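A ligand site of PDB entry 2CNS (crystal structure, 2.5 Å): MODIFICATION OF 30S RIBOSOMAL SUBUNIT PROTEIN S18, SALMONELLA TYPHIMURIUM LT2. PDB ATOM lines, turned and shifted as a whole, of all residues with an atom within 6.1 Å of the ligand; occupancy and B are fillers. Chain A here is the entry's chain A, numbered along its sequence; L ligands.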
ATOM      1  N   ALA A  22      11.556 -20.955 -14.116  1.00  0.00           N
ATOM      2  CA  ALA A  22      10.782 -21.306 -15.284  1.00  0.00           C
ATOM      3  C   ALA A  22      11.652 -21.440 -16.541  1.00  0.00           C
ATOM      4  O   ALA A  22      11.507 -22.411 -17.298  1.00  0.00           O
ATOM      5  CB  ALA A  22       9.692 -20.311 -15.508  1.00  0.00           C
ATOM      6  N   HIS A  23      12.574 -20.488 -16.743  1.00  0.00           N
ATOM      7  CA  HIS A  23      13.466 -20.428 -17.932  1.00  0.00           C
ATOM      8  C   HIS A  23      14.647 -21.382 -17.888  1.00  0.00           C
ATOM      9  O   HIS A  23      15.511 -21.308 -17.004  1.00  0.00           O
ATOM     10  CB  HIS A  23      14.000 -19.009 -18.157  1.00  0.00           C
ATOM     11  CG  HIS A  23      13.049 -18.111 -18.869  1.00  0.00           C
ATOM     12  ND1 HIS A  23      13.132 -17.876 -20.223  1.00  0.00           N
ATOM     13  CD2 HIS A  23      11.985 -17.405 -18.425  1.00  0.00           C
ATOM     14  CE1 HIS A  23      12.157 -17.049 -20.577  1.00  0.00           C
ATOM     15  NE2 HIS A  23      11.450 -16.751 -19.507  1.00  0.00           N
ATOM     16  N   ALA A  24      14.703 -22.240 -18.906  1.00  0.00           N
ATOM     17  CA  ALA A  24      15.767 -23.234 -19.041  1.00  0.00           C
ATOM     18  C   ALA A  24      17.091 -22.540 -19.314  1.00  0.00           C
ATOM     19  O   ALA A  24      18.152 -23.078 -19.010  1.00  0.00           O
ATOM     20  CB  ALA A  24      15.417 -24.231 -20.155  1.00  0.00           C
ATOM     21  N   LEU A  66       7.173  -9.032 -27.342  1.00  0.00           N
ATOM     22  CA  LEU A  66       7.105  -9.827 -26.111  1.00  0.00           C
ATOM     23  C   LEU A  66       8.515 -10.347 -25.885  1.00  0.00           C
ATOM     24  O   LEU A  66       8.950 -11.262 -26.573  1.00  0.00           O
ATOM     25  CB  LEU A  66       6.121 -10.997 -26.227  1.00  0.00           C
ATOM     26  CG  LEU A  66       6.001 -11.989 -25.053  1.00  0.00           C
ATOM     27  CD1 LEU A  66       5.457 -11.342 -23.753  1.00  0.00           C
ATOM     28  CD2 LEU A  66       5.115 -13.164 -25.412  1.00  0.00           C
ATOM     29  N   PHE A  67       9.247  -9.749 -24.956  1.00  0.00           N
ATOM     30  CA  PHE A  67      10.635 -10.183 -24.706  1.00  0.00           C
ATOM     31  C   PHE A  67      10.687 -11.399 -23.826  1.00  0.00           C
ATOM     32  O   PHE A  67      11.658 -12.110 -23.827  1.00  0.00           O
ATOM     33  CB  PHE A  67      11.435  -9.076 -24.038  1.00  0.00           C
ATOM     34  CG  PHE A  67      11.809  -7.934 -24.961  1.00  0.00           C
ATOM     35  CD1 PHE A  67      12.515  -8.177 -26.148  1.00  0.00           C
ATOM     36  CD2 PHE A  67      11.529  -6.615 -24.610  1.00  0.00           C
ATOM     37  CE1 PHE A  67      12.889  -7.088 -27.003  1.00  0.00           C
ATOM     38  CE2 PHE A  67      11.914  -5.536 -25.446  1.00  0.00           C
ATOM     39  CZ  PHE A  67      12.579  -5.775 -26.642  1.00  0.00           C
ATOM     40  N   ASN A  68       9.622 -11.629 -23.060  1.00  0.00           N
ATOM     41  CA  ASN A  68       9.611 -12.619 -22.019  1.00  0.00           C
ATOM     42  C   ASN A  68       8.193 -12.882 -21.496  1.00  0.00           C
ATOM     43  O   ASN A  68       7.446 -11.949 -21.161  1.00  0.00           O
ATOM     44  CB  ASN A  68      10.505 -12.126 -20.878  1.00  0.00           C
ATOM     45  CG  ASN A  68      10.988 -13.246 -19.974  1.00  0.00           C
ATOM     46  OD1 ASN A  68      10.418 -14.328 -19.955  1.00  0.00           O
ATOM     47  ND2 ASN A  68      12.043 -12.985 -19.206  1.00  0.00           N
ATOM     48  N   ILE A  69       7.816 -14.158 -21.440  1.00  0.00           N
ATOM     49  CA  ILE A  69       6.684 -14.603 -20.621  1.00  0.00           C
ATOM     50  C   ILE A  69       7.125 -15.856 -19.852  1.00  0.00           C
ATOM     51  O   ILE A  69       7.903 -16.685 -20.364  1.00  0.00           O
ATOM     52  CB  ILE A  69       5.398 -14.878 -21.424  1.00  0.00           C
ATOM     53  CG1 ILE A  69       4.295 -15.365 -20.457  1.00  0.00           C
ATOM     54  CG2 ILE A  69       5.672 -15.856 -22.621  1.00  0.00           C
ATOM     55  CD1 ILE A  69       2.871 -15.178 -20.978  1.00  0.00           C
ATOM     56  N   ALA A  70       6.664 -15.952 -18.614  1.00  0.00           N
ATOM     57  CA  ALA A  70       7.033 -17.057 -17.746  1.00  0.00           C
ATOM     58  C   ALA A  70       5.919 -17.335 -16.751  1.00  0.00           C
ATOM     59  O   ALA A  70       5.384 -16.433 -16.121  1.00  0.00           O
ATOM     60  CB  ALA A  70       8.312 -16.740 -17.012  1.00  0.00           C
ATOM     61  N   VAL A  71       5.573 -18.610 -16.625  1.00  0.00           N
ATOM     62  CA  VAL A  71       4.669 -19.069 -15.592  1.00  0.00           C
ATOM     63  C   VAL A  71       5.486 -19.918 -14.615  1.00  0.00           C
ATOM     64  O   VAL A  71       6.244 -20.805 -15.029  1.00  0.00           O
ATOM     65  CB  VAL A  71       3.500 -19.882 -16.199  1.00  0.00           C
ATOM     66  CG1 VAL A  71       2.592 -20.435 -15.110  1.00  0.00           C
ATOM     67  CG2 VAL A  71       2.713 -19.026 -17.217  1.00  0.00           C
ATOM     68  N   ASP A  72       5.363 -19.640 -13.329  1.00  0.00           N
ATOM     69  CA  ASP A  72       6.079 -20.433 -12.357  1.00  0.00           C
ATOM     70  C   ASP A  72       5.688 -21.905 -12.508  1.00  0.00           C
ATOM     71  O   ASP A  72       4.524 -22.195 -12.774  1.00  0.00           O
ATOM     72  CB  ASP A  72       5.782 -19.934 -10.958  1.00  0.00           C
ATOM     73  CG  ASP A  72       6.590 -20.655  -9.915  1.00  0.00           C
ATOM     74  OD1 ASP A  72       6.228 -21.809  -9.593  1.00  0.00           O
ATOM     75  OD2 ASP A  72       7.577 -20.057  -9.443  1.00  0.00           O
ATOM     76  N   PHE A  75       2.505 -23.366 -11.243  1.00  0.00           N
ATOM     77  CA  PHE A  75       1.263 -22.932 -11.888  1.00  0.00           C
ATOM     78  C   PHE A  75       1.129 -23.272 -13.370  1.00  0.00           C
ATOM     79  O   PHE A  75       0.170 -22.835 -14.011  1.00  0.00           O
ATOM     80  CB  PHE A  75       1.102 -21.425 -11.722  1.00  0.00           C
ATOM     81  CG  PHE A  75       0.769 -21.022 -10.337  1.00  0.00           C
ATOM     82  CD1 PHE A  75      -0.509 -21.212  -9.825  1.00  0.00           C
ATOM     83  CD2 PHE A  75       1.735 -20.442  -9.534  1.00  0.00           C
ATOM     84  CE1 PHE A  75      -0.818 -20.842  -8.521  1.00  0.00           C
ATOM     85  CE2 PHE A  75       1.443 -20.058  -8.240  1.00  0.00           C
ATOM     86  CZ  PHE A  75       0.157 -20.260  -7.729  1.00  0.00           C
ATOM     87  N   GLN A  76       2.059 -24.035 -13.914  1.00  0.00           N
ATOM     88  CA  GLN A  76       2.057 -24.306 -15.346  1.00  0.00           C
ATOM     89  C   GLN A  76       1.014 -25.321 -15.754  1.00  0.00           C
ATOM     90  O   GLN A  76       0.471 -26.030 -14.900  1.00  0.00           O
ATOM     91  CB  GLN A  76       3.443 -24.739 -15.826  1.00  0.00           C
ATOM     92  CG  GLN A  76       4.443 -23.574 -15.992  1.00  0.00           C
ATOM     93  CD  GLN A  76       5.817 -24.054 -16.353  1.00  0.00           C
ATOM     94  OE1 GLN A  76       6.015 -25.226 -16.636  1.00  0.00           O
ATOM     95  NE2 GLN A  76       6.789 -23.144 -16.348  1.00  0.00           N
ATOM     96  N   ARG A  77       0.762 -25.403 -17.053  1.00  0.00           N
ATOM     97  CA  ARG A  77      -0.259 -26.315 -17.638  1.00  0.00           C
ATOM     98  C   ARG A  77      -1.651 -26.154 -17.008  1.00  0.00           C
ATOM     99  O   ARG A  77      -2.459 -27.077 -17.058  1.00  0.00           O
ATOM    100  CB  ARG A  77       0.194 -27.796 -17.609  1.00  0.00           C
ATOM    101  CG  ARG A  77       1.527 -28.114 -18.343  1.00  0.00           C
ATOM    102  CD  ARG A  77       1.332 -29.190 -19.434  1.00  0.00           C
ATOM    103  NE  ARG A  77       0.445 -28.672 -20.493  1.00  0.00           N
ATOM    104  CZ  ARG A  77       0.246 -29.216 -21.702  1.00  0.00           C
ATOM    105  NH1 ARG A  77       0.890 -30.336 -22.073  1.00  0.00           N
ATOM    106  NH2 ARG A  77      -0.589 -28.628 -22.570  1.00  0.00           N
ATOM    107  N   ARG A  78      -1.928 -24.965 -16.453  1.00  0.00           N
ATOM    108  CA  ARG A  78      -3.210 -24.656 -15.810  1.00  0.00           C
ATOM    109  C   ARG A  78      -3.987 -23.587 -16.589  1.00  0.00           C
ATOM    110  O   ARG A  78      -5.083 -23.198 -16.168  1.00  0.00           O
ATOM    111  CB  ARG A  78      -3.013 -24.204 -14.344  1.00  0.00           C
ATOM    112  CG  ARG A  78      -2.840 -25.337 -13.324  1.00  0.00           C
ATOM    113  CD  ARG A  78      -2.594 -24.754 -11.924  1.00  0.00           C
ATOM    114  NE  ARG A  78      -3.046 -25.632 -10.838  1.00  0.00           N
ATOM    115  CZ  ARG A  78      -3.034 -25.313  -9.544  1.00  0.00           C
ATOM    116  NH1 ARG A  78      -2.596 -24.118  -9.135  1.00  0.00           N
ATOM    117  NH2 ARG A  78      -3.471 -26.180  -8.638  1.00  0.00           N
ATOM    118  N   GLY A  79      -3.411 -23.114 -17.704  1.00  0.00           N
ATOM    119  CA  GLY A  79      -4.070 -22.163 -18.601  1.00  0.00           C
ATOM    120  C   GLY A  79      -3.749 -20.686 -18.348  1.00  0.00           C
ATOM    121  O   GLY A  79      -4.304 -19.782 -18.969  1.00  0.00           O
ATOM    122  N   LEU A  80      -2.838 -20.455 -17.418  1.00  0.00           N
ATOM    123  CA  LEU A  80      -2.538 -19.089 -17.009  1.00  0.00           C
ATOM    124  C   LEU A  80      -1.656 -18.352 -17.990  1.00  0.00           C
ATOM    125  O   LEU A  80      -1.776 -17.148 -18.148  1.00  0.00           O
ATOM    126  CB  LEU A  80      -1.983 -19.056 -15.589  1.00  0.00           C
ATOM    127  CG  LEU A  80      -2.863 -19.864 -14.631  1.00  0.00           C
ATOM    128  CD1 LEU A  80      -2.183 -19.929 -13.287  1.00  0.00           C
ATOM    129  CD2 LEU A  80      -4.285 -19.300 -14.495  1.00  0.00           C
ATOM    130  N   GLY A  81      -0.776 -19.076 -18.681  1.00  0.00           N
ATOM    131  CA  GLY A  81       0.088 -18.422 -19.675  1.00  0.00           C
ATOM    132  C   GLY A  81      -0.762 -17.827 -20.762  1.00  0.00           C
ATOM    133  O   GLY A  81      -0.625 -16.665 -21.128  1.00  0.00           O
ATOM    134  N   ARG A  82      -1.688 -18.626 -21.264  1.00  0.00           N
ATOM    135  CA  ARG A  82      -2.623 -18.189 -22.276  1.00  0.00           C
ATOM    136  C   ARG A  82      -3.439 -16.999 -21.808  1.00  0.00           C
ATOM    137  O   ARG A  82      -3.589 -16.047 -22.556  1.00  0.00           O
ATOM    138  CB  ARG A  82      -3.563 -19.343 -22.622  1.00  0.00           C
ATOM    139  CG  ARG A  82      -4.587 -18.989 -23.665  1.00  0.00           C
ATOM    140  CD  ARG A  82      -5.542 -20.152 -23.841  1.00  0.00           C
ATOM    141  NE  ARG A  82      -5.847 -20.298 -25.252  1.00  0.00           N
ATOM    142  CZ  ARG A  82      -5.221 -21.158 -26.072  1.00  0.00           C
ATOM    143  NH1 ARG A  82      -4.266 -21.972 -25.617  1.00  0.00           N
ATOM    144  NH2 ARG A  82      -5.580 -21.197 -27.337  1.00  0.00           N
ATOM    145  N   MET A  83      -3.968 -17.045 -20.586  1.00  0.00           N
ATOM    146  CA  MET A  83      -4.818 -15.953 -20.092  1.00  0.00           C
ATOM    147  C   MET A  83      -4.050 -14.633 -19.975  1.00  0.00           C
ATOM    148  O   MET A  83      -4.567 -13.562 -20.360  1.00  0.00           O
ATOM    149  CB  MET A  83      -5.488 -16.318 -18.760  1.00  0.00           C
ATOM    150  CG  MET A  83      -6.336 -15.223 -18.095  1.00  0.00           C
ATOM    151  SD  MET A  83      -6.779 -15.702 -16.382  1.00  0.00           S
ATOM    152  CE  MET A  83      -7.907 -17.078 -16.713  1.00  0.00           C
ATOM    153  N   LEU A 102       8.040 -11.839 -31.341  1.00  0.00           N
ATOM    154  CA  LEU A 102       8.783 -12.540 -30.306  1.00  0.00           C
ATOM    155  C   LEU A 102       9.814 -13.445 -30.967  1.00  0.00           C
ATOM    156  O   LEU A 102       9.708 -13.733 -32.148  1.00  0.00           O
ATOM    157  CB  LEU A 102       7.852 -13.354 -29.377  1.00  0.00           C
ATOM    158  CG  LEU A 102       7.051 -14.569 -29.898  1.00  0.00           C
ATOM    159  CD1 LEU A 102       7.935 -15.795 -30.219  1.00  0.00           C
ATOM    160  CD2 LEU A 102       5.959 -14.994 -28.930  1.00  0.00           C
ATOM    161  N   GLU A 103      10.830 -13.847 -30.236  1.00  0.00           N
ATOM    162  CA  GLU A 103      11.617 -14.982 -30.661  1.00  0.00           C
ATOM    163  C   GLU A 103      11.626 -16.101 -29.626  1.00  0.00           C
ATOM    164  O   GLU A 103      11.486 -15.851 -28.441  1.00  0.00           O
ATOM    165  CB  GLU A 103      13.035 -14.573 -31.057  1.00  0.00           C
ATOM    166  CG  GLU A 103      13.437 -13.213 -30.630  1.00  0.00           C
ATOM    167  CD  GLU A 103      14.919 -13.003 -30.856  1.00  0.00           C
ATOM    168  OE1 GLU A 103      15.362 -13.044 -32.039  1.00  0.00           O
ATOM    169  OE2 GLU A 103      15.642 -12.794 -29.853  1.00  0.00           O
ATOM    170  N   VAL A 104      11.750 -17.337 -30.090  1.00  0.00           N
ATOM    171  CA  VAL A 104      11.700 -18.479 -29.194  1.00  0.00           C
ATOM    172  C   VAL A 104      12.689 -19.550 -29.661  1.00  0.00           C
ATOM    173  O   VAL A 104      12.970 -19.666 -30.874  1.00  0.00           O
ATOM    174  CB  VAL A 104      10.249 -19.032 -29.084  1.00  0.00           C
ATOM    175  CG1 VAL A 104       9.658 -19.347 -30.454  1.00  0.00           C
ATOM    176  CG2 VAL A 104      10.170 -20.241 -28.140  1.00  0.00           C
ATOM    177  N   ARG A 105      13.226 -20.300 -28.713  1.00  0.00           N
ATOM    178  CA  ARG A 105      14.062 -21.473 -29.021  1.00  0.00           C
ATOM    179  C   ARG A 105      13.287 -22.499 -29.836  1.00  0.00           C
ATOM    180  O   ARG A 105      12.144 -22.793 -29.491  1.00  0.00           O
ATOM    181  CB  ARG A 105      14.568 -22.121 -27.728  1.00  0.00           C
ATOM    182  CG  ARG A 105      15.725 -21.360 -27.142  1.00  0.00           C
ATOM    183  CD  ARG A 105      16.056 -21.707 -25.693  1.00  0.00           C
ATOM    184  NE  ARG A 105      17.154 -20.839 -25.222  1.00  0.00           N
ATOM    185  CZ  ARG A 105      18.453 -21.084 -25.432  1.00  0.00           C
ATOM    186  NH1 ARG A 105      18.838 -22.191 -26.077  1.00  0.00           N
ATOM    187  NH2 ARG A 105      19.371 -20.233 -24.978  1.00  0.00           N
ATOM    188  N   ASN A 108      11.737 -25.117 -27.605  1.00  0.00           N
ATOM    189  CA  ASN A 108      10.742 -24.798 -26.628  1.00  0.00           C
ATOM    190  C   ASN A 108       9.372 -25.159 -27.172  1.00  0.00           C
ATOM    191  O   ASN A 108       8.602 -24.288 -27.569  1.00  0.00           O
ATOM    192  CB  ASN A 108      10.826 -23.344 -26.230  1.00  0.00           C
ATOM    193  CG  ASN A 108      10.060 -23.034 -24.948  1.00  0.00           C
ATOM    194  OD1 ASN A 108       9.139 -23.771 -24.557  1.00  0.00           O
ATOM    195  ND2 ASN A 108      10.427 -21.942 -24.311  1.00  0.00           N
ATOM    196  N   ALA A 109       9.120 -26.463 -27.180  1.00  0.00           N
ATOM    197  CA  ALA A 109       7.841 -27.069 -27.585  1.00  0.00           C
ATOM    198  C   ALA A 109       6.621 -26.384 -26.969  1.00  0.00           C
ATOM    199  O   ALA A 109       5.652 -26.088 -27.665  1.00  0.00           O
ATOM    200  CB  ALA A 109       7.837 -28.565 -27.216  1.00  0.00           C
ATOM    201  N   ALA A 110       6.675 -26.140 -25.669  1.00  0.00           N
ATOM    202  CA  ALA A 110       5.522 -25.611 -24.940  1.00  0.00           C
ATOM    203  C   ALA A 110       5.221 -24.172 -25.324  1.00  0.00           C
ATOM    204  O   ALA A 110       4.067 -23.805 -25.523  1.00  0.00           O
ATOM    205  CB  ALA A 110       5.735 -25.715 -23.457  1.00  0.00           C
ATOM    206  N   ALA A 111       6.255 -23.349 -25.424  1.00  0.00           N
ATOM    207  CA  ALA A 111       6.052 -21.956 -25.793  1.00  0.00           C
ATOM    208  C   ALA A 111       5.489 -21.869 -27.198  1.00  0.00           C
ATOM    209  O   ALA A 111       4.529 -21.126 -27.436  1.00  0.00           O
ATOM    210  CB  ALA A 111       7.338 -21.164 -25.700  1.00  0.00           C
ATOM    211  N   ALA A 113       3.779 -23.934 -28.855  1.00  0.00           N
ATOM    212  CA  ALA A 113       2.401 -24.387 -28.942  1.00  0.00           C
ATOM    213  C   ALA A 113       1.425 -23.335 -28.436  1.00  0.00           C
ATOM    214  O   ALA A 113       0.361 -23.129 -29.034  1.00  0.00           O
ATOM    215  CB  ALA A 113       2.196 -25.727 -28.232  1.00  0.00           C
ATOM    216  N   LEU A 114       1.782 -22.650 -27.345  1.00  0.00           N
ATOM    217  CA  LEU A 114       0.980 -21.539 -26.871  1.00  0.00           C
ATOM    218  C   LEU A 114       0.876 -20.472 -27.986  1.00  0.00           C
ATOM    219  O   LEU A 114      -0.226 -20.069 -28.375  1.00  0.00           O
ATOM    220  CB  LEU A 114       1.599 -20.962 -25.610  1.00  0.00           C
ATOM    221  CG  LEU A 114       1.108 -19.580 -25.162  1.00  0.00           C
ATOM    222  CD1 LEU A 114      -0.280 -19.638 -24.582  1.00  0.00           C
ATOM    223  CD2 LEU A 114       2.065 -18.990 -24.148  1.00  0.00           C
ATOM    224  N   TYR A 115       2.012 -20.090 -28.537  1.00  0.00           N
ATOM    225  CA  TYR A 115       2.034 -19.038 -29.546  1.00  0.00           C
ATOM    226  C   TYR A 115       1.223 -19.424 -30.764  1.00  0.00           C
ATOM    227  O   TYR A 115       0.385 -18.642 -31.223  1.00  0.00           O
ATOM    228  CB  TYR A 115       3.463 -18.638 -29.933  1.00  0.00           C
ATOM    229  CG  TYR A 115       4.325 -18.263 -28.746  1.00  0.00           C
ATOM    230  CD1 TYR A 115       3.780 -17.628 -27.616  1.00  0.00           C
ATOM    231  CD2 TYR A 115       5.684 -18.539 -28.748  1.00  0.00           C
ATOM    232  CE1 TYR A 115       4.586 -17.299 -26.530  1.00  0.00           C
ATOM    233  CE2 TYR A 115       6.498 -18.196 -27.692  1.00  0.00           C
ATOM    234  CZ  TYR A 115       5.958 -17.600 -26.584  1.00  0.00           C
ATOM    235  OH  TYR A 115       6.800 -17.304 -25.530  1.00  0.00           O
ATOM    236  N   SER A 117      -1.091 -21.477 -30.925  1.00  0.00           N
ATOM    237  CA  SER A 117      -2.510 -21.560 -30.586  1.00  0.00           C
ATOM    238  C   SER A 117      -3.178 -20.188 -30.504  1.00  0.00           C
ATOM    239  O   SER A 117      -4.390 -20.093 -30.703  1.00  0.00           O
ATOM    240  CB  SER A 117      -2.787 -22.378 -29.321  1.00  0.00           C
ATOM    241  OG  SER A 117      -2.814 -21.563 -28.166  1.00  0.00           O
HETATM  242  N1  LIG L   1       3.754 -29.265 -23.657  1.00  0.00           N
HETATM  243  C1  LIG L   1       3.043 -29.104 -24.735  1.00  0.00           C
HETATM  244  N2  LIG L   1       2.236 -28.097 -24.896  1.00  0.00           N
HETATM  245  C2  LIG L   1       2.111 -27.196 -23.965  1.00  0.00           C
HETATM  246  C3  LIG L   1       2.827 -27.318 -22.825  1.00  0.00           C
HETATM  247  C4  LIG L   1       3.664 -28.390 -22.688  1.00  0.00           C
HETATM  248  N3  LIG L   1       4.357 -28.494 -21.567  1.00  0.00           N
HETATM  249  N4  LIG L   1       2.560 -26.301 -22.037  1.00  0.00           N
HETATM  250  C5  LIG L   1       1.706 -25.563 -22.698  1.00  0.00           C
HETATM  251  N5  LIG L   1       1.428 -26.111 -23.855  1.00  0.00           N
HETATM  252  C6  LIG L   1       0.587 -25.561 -24.814  1.00  0.00           C
HETATM  253  C7  LIG L   1      -0.780 -26.037 -25.022  1.00  0.00           C
HETATM  254  O1  LIG L   1      -1.219 -25.554 -26.254  1.00  0.00           O
HETATM  255  C8  LIG L   1      -1.515 -25.295 -23.984  1.00  0.00           C
HETATM  256  O2  LIG L   1      -2.743 -25.084 -24.588  1.00  0.00           O
HETATM  257  P1  LIG L   1      -3.942 -26.036 -24.659  1.00  0.00           P
HETATM  258  O3  LIG L   1      -4.195 -25.744 -26.193  1.00  0.00           O
HETATM  259  O4  LIG L   1      -4.922 -25.297 -23.746  1.00  0.00           O
HETATM  260  O5  LIG L   1      -3.771 -27.416 -24.249  1.00  0.00           O
HETATM  261  C9  LIG L   1      -0.802 -23.966 -24.056  1.00  0.00           C
HETATM  262  O6  LIG L   1       0.506 -24.276 -24.369  1.00  0.00           O
HETATM  263  C10 LIG L   1      -0.909 -22.969 -22.932  1.00  0.00           C
HETATM  264  O7  LIG L   1      -1.014 -23.534 -21.751  1.00  0.00           O
HETATM  265  P2  LIG L   1      -0.846 -22.799 -20.614  1.00  0.00           P
HETATM  266  O8  LIG L   1      -1.556 -21.644 -20.830  1.00  0.00           O
HETATM  267  O9  LIG L   1      -1.299 -23.683 -19.638  1.00  0.00           O
HETATM  268  O10 LIG L   1       0.634 -22.605 -20.520  1.00  0.00           O
HETATM  269  P3  LIG L   1       1.389 -22.326 -19.374  1.00  0.00           P
HETATM  270  O11 LIG L   1       0.706 -21.613 -18.438  1.00  0.00           O
HETATM  271  O12 LIG L   1       2.065 -23.444 -18.985  1.00  0.00           O
HETATM  272  O13 LIG L   1       2.375 -21.425 -19.800  1.00  0.00           O
HETATM  273  C11 LIG L   1       4.675 -21.150 -20.703  1.00  0.00           C
HETATM  274  C12 LIG L   1       3.236 -21.609 -20.869  1.00  0.00           C
HETATM  275  C13 LIG L   1       5.359 -21.514 -21.975  1.00  0.00           C
HETATM  276  C14 LIG L   1       4.790 -19.660 -20.565  1.00  0.00           C
HETATM  277  C15 LIG L   1       5.364 -21.875 -19.537  1.00  0.00           C
HETATM  278  O14 LIG L   1       5.570 -23.172 -19.945  1.00  0.00           O
HETATM  279  C16 LIG L   1       6.717 -21.350 -19.116  1.00  0.00           C
HETATM  280  O15 LIG L   1       6.857 -20.473 -18.313  1.00  0.00           O
HETATM  281  N6  LIG L   1       7.849 -21.990 -19.689  1.00  0.00           N
HETATM  282  C17 LIG L   1       9.244 -21.678 -19.338  1.00  0.00           C
HETATM  283  C18 LIG L   1       9.516 -20.213 -19.675  1.00  0.00           C
HETATM  284  C19 LIG L   1       9.568 -20.056 -21.201  1.00  0.00           C
HETATM  285  O16 LIG L   1      10.149 -20.876 -21.919  1.00  0.00           O
HETATM  286  N7  LIG L   1       8.956 -18.966 -21.653  1.00  0.00           N
HETATM  287  C20 LIG L   1       8.922 -18.644 -23.081  1.00  0.00           C
HETATM  288  C21 LIG L   1      10.271 -17.991 -23.495  1.00  0.00           C
HETATM  289  S1  LIG L   1      10.148 -17.317 -25.197  1.00  0.00           S
HETATM  290  C22 LIG L   1       9.647 -15.680 -24.808  1.00  0.00           C
HETATM  291  O17 LIG L   1       9.568 -15.370 -23.612  1.00  0.00           O
HETATM  292  C23 LIG L   1       9.317 -14.658 -25.920  1.00  0.00           C
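Residues that only touch the ligand: Ala 22, His 23, Leu 66, Phe 67, Asn 68, Ala 70, Leu 80, Leu 102, Glu 103, Ala 110, Ala 111, Ala 113 and Leu 114. Hydrophobic or aromatic side chains within 4 Å of the ligand: Ala 22, His 23, Val 71, Leu 102, Ala 110, Ala 111, Ala 113 and Leu 114. 23 residues have an atom within 4 Å of the ligand: Ala 22, His 23, Leu 66, Phe 67, Asn 68, Ile 69, Ala 70, Val 71, Gln 76, Arg 77, Arg 78, Gly 79, Leu 80, Gly 81, Arg 82, Leu 102, Glu 103, Asn 108, Ala 110, Ala 111, Ala 113, Leu 114 and Tyr 115. Along chain A the residues within 4 Å of the ligand span positions 22 to 115.
NH2 of Arg 82 lies within hydrogen-bond range of OG of Ser 117, 2.9 Å away. The backbone carbonyl oxygen of Leu 114 lies within hydrogen-bond range of the side-chain hydroxyl of Ser 117 (3.0 Å). The side-chain amide oxygen (OD1) of Asn 108 lies within hydrogen-bond range of the backbone NH (N) of Ala 111 (3.0 Å). A ring nitrogen (NE2) of His 23 lies within hydrogen-bond range of the side-chain amide oxygen of Asn 68. NE2 of Gln 76 is in hydrogen-bond range of O of Val 71 (2.7 Å).
N of Arg 78 lies within hydrogen-bond range of O9 of the ligand, at 3.5 Å. O5 of the ligand lies within salt-bridge range of NH2 of Arg 77 (3.8 Å). N of Arg 82 sits at hydrogen-bond distance from O8 of the ligand (3.1 Å). An oxygen (O3) of the ligand is in salt-bridge range of the guanidinium group (NH1) of Arg 82, 3.8 Å away. The backbone NH (N) of Val 71 sits at hydrogen-bond distance from an oxygen (O15) of the ligand (2.8 Å). An oxygen (O9) of the ligand sits at hydrogen-bond distance from the backbone NH (N) of Gly 79, at 2.9 Å. The backbone NH (N) of Ile 69 sits at hydrogen-bond distance from an oxygen (O17) of the ligand (3.0 Å). The backbone carbonyl oxygen of Ile 69 sits at hydrogen-bond distance from a nitrogen (N7) of the ligand (2.8 Å). The side-chain hydroxyl of Tyr 115 lies close to a sulfur (S1) of the ligand (3.4 Å). The backbone NH (N) of Gly 81 lies within hydrogen-bond range of an oxygen (O11) of the ligand, at 2.9 Å. ND2 of Asn 108 lies within hydrogen-bond range of O16 of the ligand, at 2.6 Å. The backbone NH (N) of Arg 77 is in hydrogen-bond range of an oxygen (O12) of the ligand (3.0 Å). NE2 of Gln 76 sits close to O15 of the ligand, 3.3 Å away.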
